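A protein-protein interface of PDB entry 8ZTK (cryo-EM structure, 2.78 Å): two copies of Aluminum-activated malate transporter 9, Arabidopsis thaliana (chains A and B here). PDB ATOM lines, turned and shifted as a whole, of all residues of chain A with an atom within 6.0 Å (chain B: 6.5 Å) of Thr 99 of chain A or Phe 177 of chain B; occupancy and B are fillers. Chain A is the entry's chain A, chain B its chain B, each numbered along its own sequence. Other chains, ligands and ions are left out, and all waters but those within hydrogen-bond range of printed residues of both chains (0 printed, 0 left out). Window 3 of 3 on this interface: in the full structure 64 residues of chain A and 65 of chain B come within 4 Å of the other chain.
Of the 13 printed residues of chain A, 6 touch a printed residue of chain B.
Printed residues of chain A that touch a printed residue of chain B: Ser 91, Ala 92, Gly 95, Leu 96, Thr 99 and Leu 103.
Hydrophobic or aromatic side chains of chain A within 4 Å of the printed part of chain B: Leu 103.
Hydrophobic or aromatic side chains of chain B within 4 Å of the printed part of chain A: Phe 177 and Phe 181.
Among the printed residues, 8 pairs touch across the chains.
Among the printed residues, no Asp or Glu carboxylate lies within 4 Å of a Lys or Arg side-chain nitrogen of the other chain.
OG1 of Thr 99 of chain A lies within hydrogen-bond range of O of Gly 95 of chain A, 3.4 Å away.
Among the printed residues, merely in contact across the chains: Thr 99 of chain A with Phe 177 of chain B (3.4 Å), Gly 95 of chain A with Phe 177 of chain B (3.6 Å), Ser 91 of chain A with Phe 181 of chain B (3.7 Å), Leu 96 of chain A with Phe 177 of chain B (3.8 Å), Ala 92 of chain A with Phe 181 of chain B (3.8 Å), Leu 103 of chain A with Thr 173 of chain B (3.9 Å) and Ala 92 of chain A with Phe 177 of chain B (3.9 Å).
No position is printed for both chains.
Of the 8 pairs that touch across the chains among the printed residues, none has its exchanged pair printed and touching as well.
Of the printed residues of chain B, Ala 92 of chain A touches Phe 177 (3.9 Å) and Phe 181 (3.8 Å).
Printed residues of chain B within 4 Å of Gly 95 of chain A: Phe 177.
Of the printed residues of chain B, Leu 96 of chain A touches Phe 177 (3.8 Å).
Of chain B, only Thr 173 and Phe 177 come within 4 Å of Thr 99 of chain A.
Printed residues of chain B within 4 Å of Leu 103 of chain A: Thr 173 (3.9 Å).
Of the printed residues of chain A, Thr 173 of chain B touches Thr 99 (3.2 Å) and Leu 103 (3.9 Å).
Of chain A, only Ala 92, Gly 95, Leu 96 and Thr 99 come within 4 Å of Phe 177 of chain B.
Gly 180 of chain B touches none of the printed residues of chain A.
The nearest residue of chain B that does not touch Thr 99 of chain A is Ile 176 of chain B (4.4 Å).
O of Thr 173 of chain B is in hydrogen-bond range of OG1 of Thr 99 of chain A (3.2 Å).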
ATOM      1  N   SER A  91     -30.702 -26.936  25.192  1.00  0.00           N
ATOM      2  CA  SER A  91     -30.121 -28.084  24.505  1.00  0.00           C
ATOM      3  C   SER A  91     -29.924 -27.822  23.017  1.00  0.00           C
ATOM      4  O   SER A  91     -28.912 -28.251  22.440  1.00  0.00           O
ATOM      5  CB  SER A  91     -31.002 -29.312  24.721  1.00  0.00           C
ATOM      6  OG  SER A  91     -31.404 -29.407  26.074  1.00  0.00           O
ATOM      7  N   ALA A  92     -30.806 -27.034  22.396  1.00  0.00           N
ATOM      8  CA  ALA A  92     -30.591 -26.718  20.993  1.00  0.00           C
ATOM      9  C   ALA A  92     -29.540 -25.635  20.817  1.00  0.00           C
ATOM     10  O   ALA A  92     -28.888 -25.586  19.770  1.00  0.00           O
ATOM     11  CB  ALA A  92     -31.902 -26.285  20.338  1.00  0.00           C
ATOM     12  N   ILE A  94     -26.742 -25.584  22.690  1.00  0.00           N
ATOM     13  CA  ILE A  94     -25.491 -26.334  22.738  1.00  0.00           C
ATOM     14  C   ILE A  94     -25.301 -27.134  21.453  1.00  0.00           C
ATOM     15  O   ILE A  94     -24.185 -27.222  20.919  1.00  0.00           O
ATOM     16  CB  ILE A  94     -25.451 -27.233  23.986  1.00  0.00           C
ATOM     17  CG1 ILE A  94     -25.312 -26.375  25.244  1.00  0.00           C
ATOM     18  CG2 ILE A  94     -24.312 -28.237  23.886  1.00  0.00           C
ATOM     19  CD1 ILE A  94     -24.980 -27.160  26.483  1.00  0.00           C
ATOM     20  N   GLY A  95     -26.383 -27.712  20.922  1.00  0.00           N
ATOM     21  CA  GLY A  95     -26.271 -28.391  19.642  1.00  0.00           C
ATOM     22  C   GLY A  95     -25.817 -27.468  18.525  1.00  0.00           C
ATOM     23  O   GLY A  95     -24.977 -27.840  17.699  1.00  0.00           O
ATOM     24  N   LEU A  96     -26.337 -26.237  18.503  1.00  0.00           N
ATOM     25  CA  LEU A  96     -25.937 -25.289  17.468  1.00  0.00           C
ATOM     26  C   LEU A  96     -24.477 -24.883  17.621  1.00  0.00           C
ATOM     27  O   LEU A  96     -23.751 -24.763  16.625  1.00  0.00           O
ATOM     28  CB  LEU A  96     -26.843 -24.059  17.508  1.00  0.00           C
ATOM     29  CG  LEU A  96     -26.604 -22.992  16.438  1.00  0.00           C
ATOM     30  CD1 LEU A  96     -27.091 -23.470  15.081  1.00  0.00           C
ATOM     31  CD2 LEU A  96     -27.279 -21.687  16.825  1.00  0.00           C
ATOM     32  N   ALA A  97     -24.019 -24.684  18.860  1.00  0.00           N
ATOM     33  CA  ALA A  97     -22.623 -24.306  19.056  1.00  0.00           C
ATOM     34  C   ALA A  97     -21.689 -25.422  18.600  1.00  0.00           C
ATOM     35  O   ALA A  97     -20.664 -25.164  17.948  1.00  0.00           O
ATOM     36  CB  ALA A  97     -22.371 -23.958  20.522  1.00  0.00           C
ATOM     37  N   LEU A  98     -22.046 -26.673  18.899  1.00  0.00           N
ATOM     38  CA  LEU A  98     -21.208 -27.780  18.450  1.00  0.00           C
ATOM     39  C   LEU A  98     -21.221 -27.897  16.932  1.00  0.00           C
ATOM     40  O   LEU A  98     -20.175 -28.137  16.315  1.00  0.00           O
ATOM     41  CB  LEU A  98     -21.664 -29.090  19.092  1.00  0.00           C
ATOM     42  CG  LEU A  98     -21.276 -29.340  20.550  1.00  0.00           C
ATOM     43  CD1 LEU A  98     -21.897 -30.636  21.046  1.00  0.00           C
ATOM     44  CD2 LEU A  98     -19.767 -29.368  20.712  1.00  0.00           C
ATOM     45  N   THR A  99     -22.384 -27.699  16.302  1.00  0.00           N
ATOM     46  CA  THR A  99     -22.436 -27.819  14.851  1.00  0.00           C
ATOM     47  C   THR A  99     -21.716 -26.672  14.156  1.00  0.00           C
ATOM     48  O   THR A  99     -21.190 -26.860  13.054  1.00  0.00           O
ATOM     49  CB  THR A  99     -23.892 -27.881  14.384  1.00  0.00           C
ATOM     50  OG1 THR A  99     -24.407 -29.201  14.590  1.00  0.00           O
ATOM     51  CG2 THR A  99     -23.996 -27.531  12.910  1.00  0.00           C
ATOM     52  N   ILE A 100     -21.553 -25.536  14.831  1.00  0.00           N
ATOM     53  CA  ILE A 100     -20.805 -24.434  14.236  1.00  0.00           C
ATOM     54  C   ILE A 100     -19.308 -24.684  14.353  1.00  0.00           C
ATOM     55  O   ILE A 100     -18.549 -24.466  13.398  1.00  0.00           O
ATOM     56  CB  ILE A 100     -21.209 -23.094  14.878  1.00  0.00           C
ATOM     57  CG1 ILE A 100     -22.693 -22.814  14.646  1.00  0.00           C
ATOM     58  CG2 ILE A 100     -20.357 -21.961  14.326  1.00  0.00           C
ATOM     59  CD1 ILE A 100     -23.139 -21.458  15.138  1.00  0.00           C
ATOM     60  N   VAL A 101     -18.852 -25.100  15.537  1.00  0.00           N
ATOM     61  CA  VAL A 101     -17.448 -25.482  15.667  1.00  0.00           C
ATOM     62  C   VAL A 101     -17.096 -26.578  14.665  1.00  0.00           C
ATOM     63  O   VAL A 101     -15.998 -26.588  14.097  1.00  0.00           O
ATOM     64  CB  VAL A 101     -17.132 -25.909  17.113  1.00  0.00           C
ATOM     65  CG1 VAL A 101     -15.788 -26.610  17.170  1.00  0.00           C
ATOM     66  CG2 VAL A 101     -17.130 -24.700  18.028  1.00  0.00           C
ATOM     67  N   ALA A 102     -18.021 -27.515  14.425  1.00  0.00           N
ATOM     68  CA  ALA A 102     -17.772 -28.558  13.431  1.00  0.00           C
ATOM     69  C   ALA A 102     -17.689 -27.989  12.018  1.00  0.00           C
ATOM     70  O   ALA A 102     -16.796 -28.363  11.244  1.00  0.00           O
ATOM     71  CB  ALA A 102     -18.857 -29.630  13.514  1.00  0.00           C
ATOM     72  N   LEU A 103     -18.612 -27.091  11.656  1.00  0.00           N
ATOM     73  CA  LEU A 103     -18.582 -26.514  10.316  1.00  0.00           C
ATOM     74  C   LEU A 103     -17.282 -25.762  10.069  1.00  0.00           C
ATOM     75  O   LEU A 103     -16.687 -25.878   8.991  1.00  0.00           O
ATOM     76  CB  LEU A 103     -19.779 -25.587  10.105  1.00  0.00           C
ATOM     77  CG  LEU A 103     -21.114 -26.249   9.759  1.00  0.00           C
ATOM     78  CD1 LEU A 103     -22.216 -25.208   9.671  1.00  0.00           C
ATOM     79  CD2 LEU A 103     -20.998 -27.020   8.455  1.00  0.00           C
ATOM     80  N   LEU A 104     -16.821 -24.986  11.051  1.00  0.00           N
ATOM     81  CA  LEU A 104     -15.599 -24.218  10.830  1.00  0.00           C
ATOM     82  C   LEU A 104     -14.351 -25.087  10.725  1.00  0.00           C
ATOM     83  O   LEU A 104     -13.250 -24.536  10.607  1.00  0.00           O
ATOM     84  CB  LEU A 104     -15.405 -23.187  11.944  1.00  0.00           C
ATOM     85  CG  LEU A 104     -16.558 -22.221  12.211  1.00  0.00           C
ATOM     86  CD1 LEU A 104     -16.526 -21.741  13.652  1.00  0.00           C
ATOM     87  CD2 LEU A 104     -16.491 -21.045  11.250  1.00  0.00           C
ATOM     88  N   CYS B 172     -22.769 -35.803   8.775  1.00  0.00           N
ATOM     89  CA  CYS B 172     -22.057 -35.762  10.046  1.00  0.00           C
ATOM     90  C   CYS B 172     -22.486 -34.551  10.865  1.00  0.00           C
ATOM     91  O   CYS B 172     -22.774 -34.664  12.065  1.00  0.00           O
ATOM     92  CB  CYS B 172     -20.549 -35.742   9.797  1.00  0.00           C
ATOM     93  SG  CYS B 172     -19.791 -37.376   9.646  1.00  0.00           S
ATOM     94  N   THR B 173     -22.469 -33.368  10.243  1.00  0.00           N
ATOM     95  CA  THR B 173     -22.864 -32.158  10.952  1.00  0.00           C
ATOM     96  C   THR B 173     -24.317 -32.221  11.408  1.00  0.00           C
ATOM     97  O   THR B 173     -24.685 -31.570  12.391  1.00  0.00           O
ATOM     98  CB  THR B 173     -22.638 -30.933  10.066  1.00  0.00           C
ATOM     99  OG1 THR B 173     -21.464 -31.131   9.268  1.00  0.00           O
ATOM    100  CG2 THR B 173     -22.456 -29.686  10.916  1.00  0.00           C
ATOM    101  N   LEU B 174     -25.155 -32.998  10.717  1.00  0.00           N
ATOM    102  CA  LEU B 174     -26.553 -33.115  11.108  1.00  0.00           C
ATOM    103  C   LEU B 174     -26.770 -34.170  12.181  1.00  0.00           C
ATOM    104  O   LEU B 174     -27.815 -34.159  12.842  1.00  0.00           O
ATOM    105  CB  LEU B 174     -27.422 -33.445   9.891  1.00  0.00           C
ATOM    106  CG  LEU B 174     -28.278 -32.303   9.341  1.00  0.00           C
ATOM    107  CD1 LEU B 174     -29.356 -31.916  10.341  1.00  0.00           C
ATOM    108  CD2 LEU B 174     -27.411 -31.105   8.987  1.00  0.00           C
ATOM    109  N   SER B 175     -25.812 -35.074  12.361  1.00  0.00           N
ATOM    110  CA  SER B 175     -25.893 -36.061  13.429  1.00  0.00           C
ATOM    111  C   SER B 175     -25.298 -35.538  14.727  1.00  0.00           C
ATOM    112  O   SER B 175     -25.784 -35.878  15.816  1.00  0.00           O
ATOM    113  CB  SER B 175     -25.176 -37.349  13.018  1.00  0.00           C
ATOM    114  OG  SER B 175     -23.899 -37.064  12.477  1.00  0.00           O
ATOM    115  N   ILE B 176     -24.257 -34.707  14.625  1.00  0.00           N
ATOM    116  CA  ILE B 176     -23.670 -34.096  15.814  1.00  0.00           C
ATOM    117  C   ILE B 176     -24.677 -33.200  16.522  1.00  0.00           C
ATOM    118  O   ILE B 176     -24.710 -33.150  17.756  1.00  0.00           O
ATOM    119  CB  ILE B 176     -22.394 -33.318  15.440  1.00  0.00           C
ATOM    120  CG1 ILE B 176     -21.363 -34.255  14.808  1.00  0.00           C
ATOM    121  CG2 ILE B 176     -21.823 -32.613  16.658  1.00  0.00           C
ATOM    122  CD1 ILE B 176     -19.947 -33.729  14.858  1.00  0.00           C
ATOM    123  N   PHE B 177     -25.552 -32.531  15.766  1.00  0.00           N
ATOM    124  CA  PHE B 177     -26.558 -31.678  16.391  1.00  0.00           C
ATOM    125  C   PHE B 177     -27.559 -32.500  17.192  1.00  0.00           C
ATOM    126  O   PHE B 177     -27.900 -32.143  18.327  1.00  0.00           O
ATOM    127  CB  PHE B 177     -27.274 -30.850  15.320  1.00  0.00           C
ATOM    128  CG  PHE B 177     -28.377 -29.975  15.855  1.00  0.00           C
ATOM    129  CD1 PHE B 177     -29.638 -30.492  16.103  1.00  0.00           C
ATOM    130  CD2 PHE B 177     -28.154 -28.633  16.102  1.00  0.00           C
ATOM    131  CE1 PHE B 177     -30.648 -29.693  16.594  1.00  0.00           C
ATOM    132  CE2 PHE B 177     -29.162 -27.828  16.593  1.00  0.00           C
ATOM    133  CZ  PHE B 177     -30.411 -28.359  16.838  1.00  0.00           C
ATOM    134  N   CYS B 178     -28.018 -33.622  16.636  1.00  0.00           N
ATOM    135  CA  CYS B 178     -29.012 -34.428  17.334  1.00  0.00           C
ATOM    136  C   CYS B 178     -28.408 -35.142  18.532  1.00  0.00           C
ATOM    137  O   CYS B 178     -29.068 -35.275  19.572  1.00  0.00           O
ATOM    138  CB  CYS B 178     -29.640 -35.437  16.373  1.00  0.00           C
ATOM    139  SG  CYS B 178     -30.105 -34.747  14.771  1.00  0.00           S
ATOM    140  N   ILE B 179     -27.140 -35.548  18.438  1.00  0.00           N
ATOM    141  CA  ILE B 179     -26.509 -36.172  19.594  1.00  0.00           C
ATOM    142  C   ILE B 179     -26.261 -35.142  20.687  1.00  0.00           C
ATOM    143  O   ILE B 179     -26.460 -35.423  21.874  1.00  0.00           O
ATOM    144  CB  ILE B 179     -25.212 -36.888  19.178  1.00  0.00           C
ATOM    145  CG1 ILE B 179     -25.504 -37.914  18.082  1.00  0.00           C
ATOM    146  CG2 ILE B 179     -24.568 -37.557  20.380  1.00  0.00           C
ATOM    147  CD1 ILE B 179     -26.438 -39.022  18.519  1.00  0.00           C
ATOM    148  N   GLY B 180     -25.871 -33.921  20.311  1.00  0.00           N
ATOM    149  CA  GLY B 180     -25.708 -32.882  21.311  1.00  0.00           C
ATOM    150  C   GLY B 180     -27.015 -32.543  21.995  1.00  0.00           C
ATOM    151  O   GLY B 180     -27.068 -32.385  23.219  1.00  0.00           O
ATOM    152  N   PHE B 181     -28.108 -32.511  21.226  1.00  0.00           N
ATOM    153  CA  PHE B 181     -29.397 -32.182  21.819  1.00  0.00           C
ATOM    154  C   PHE B 181     -29.852 -33.277  22.771  1.00  0.00           C
ATOM    155  O   PHE B 181     -30.300 -32.984  23.886  1.00  0.00           O
ATOM    156  CB  PHE B 181     -30.442 -31.948  20.728  1.00  0.00           C
ATOM    157  CG  PHE B 181     -31.830 -31.708  21.260  1.00  0.00           C
ATOM    158  CD1 PHE B 181     -32.667 -32.771  21.564  1.00  0.00           C
ATOM    159  CD2 PHE B 181     -32.293 -30.422  21.467  1.00  0.00           C
ATOM    160  CE1 PHE B 181     -33.937 -32.552  22.061  1.00  0.00           C
ATOM    161  CE2 PHE B 181     -33.563 -30.196  21.962  1.00  0.00           C
ATOM    162  CZ  PHE B 181     -34.385 -31.263  22.259  1.00  0.00           C
ATOM    163  N   LEU B 182     -29.723 -34.545  22.372  1.00  0.00           N
ATOM    164  CA  LEU B 182     -30.225 -35.600  23.245  1.00  0.00           C
ATOM    165  C   LEU B 182     -29.339 -35.771  24.472  1.00  0.00           C
ATOM    166  O   LEU B 182     -29.850 -36.018  25.575  1.00  0.00           O
ATOM    167  CB  LEU B 182     -30.335 -36.917  22.478  1.00  0.00           C
ATOM    168  CG  LEU B 182     -31.383 -36.972  21.364  1.00  0.00           C
ATOM    169  CD1 LEU B 182     -31.030 -38.042  20.343  1.00  0.00           C
ATOM    170  CD2 LEU B 182     -32.768 -37.213  21.941  1.00  0.00           C
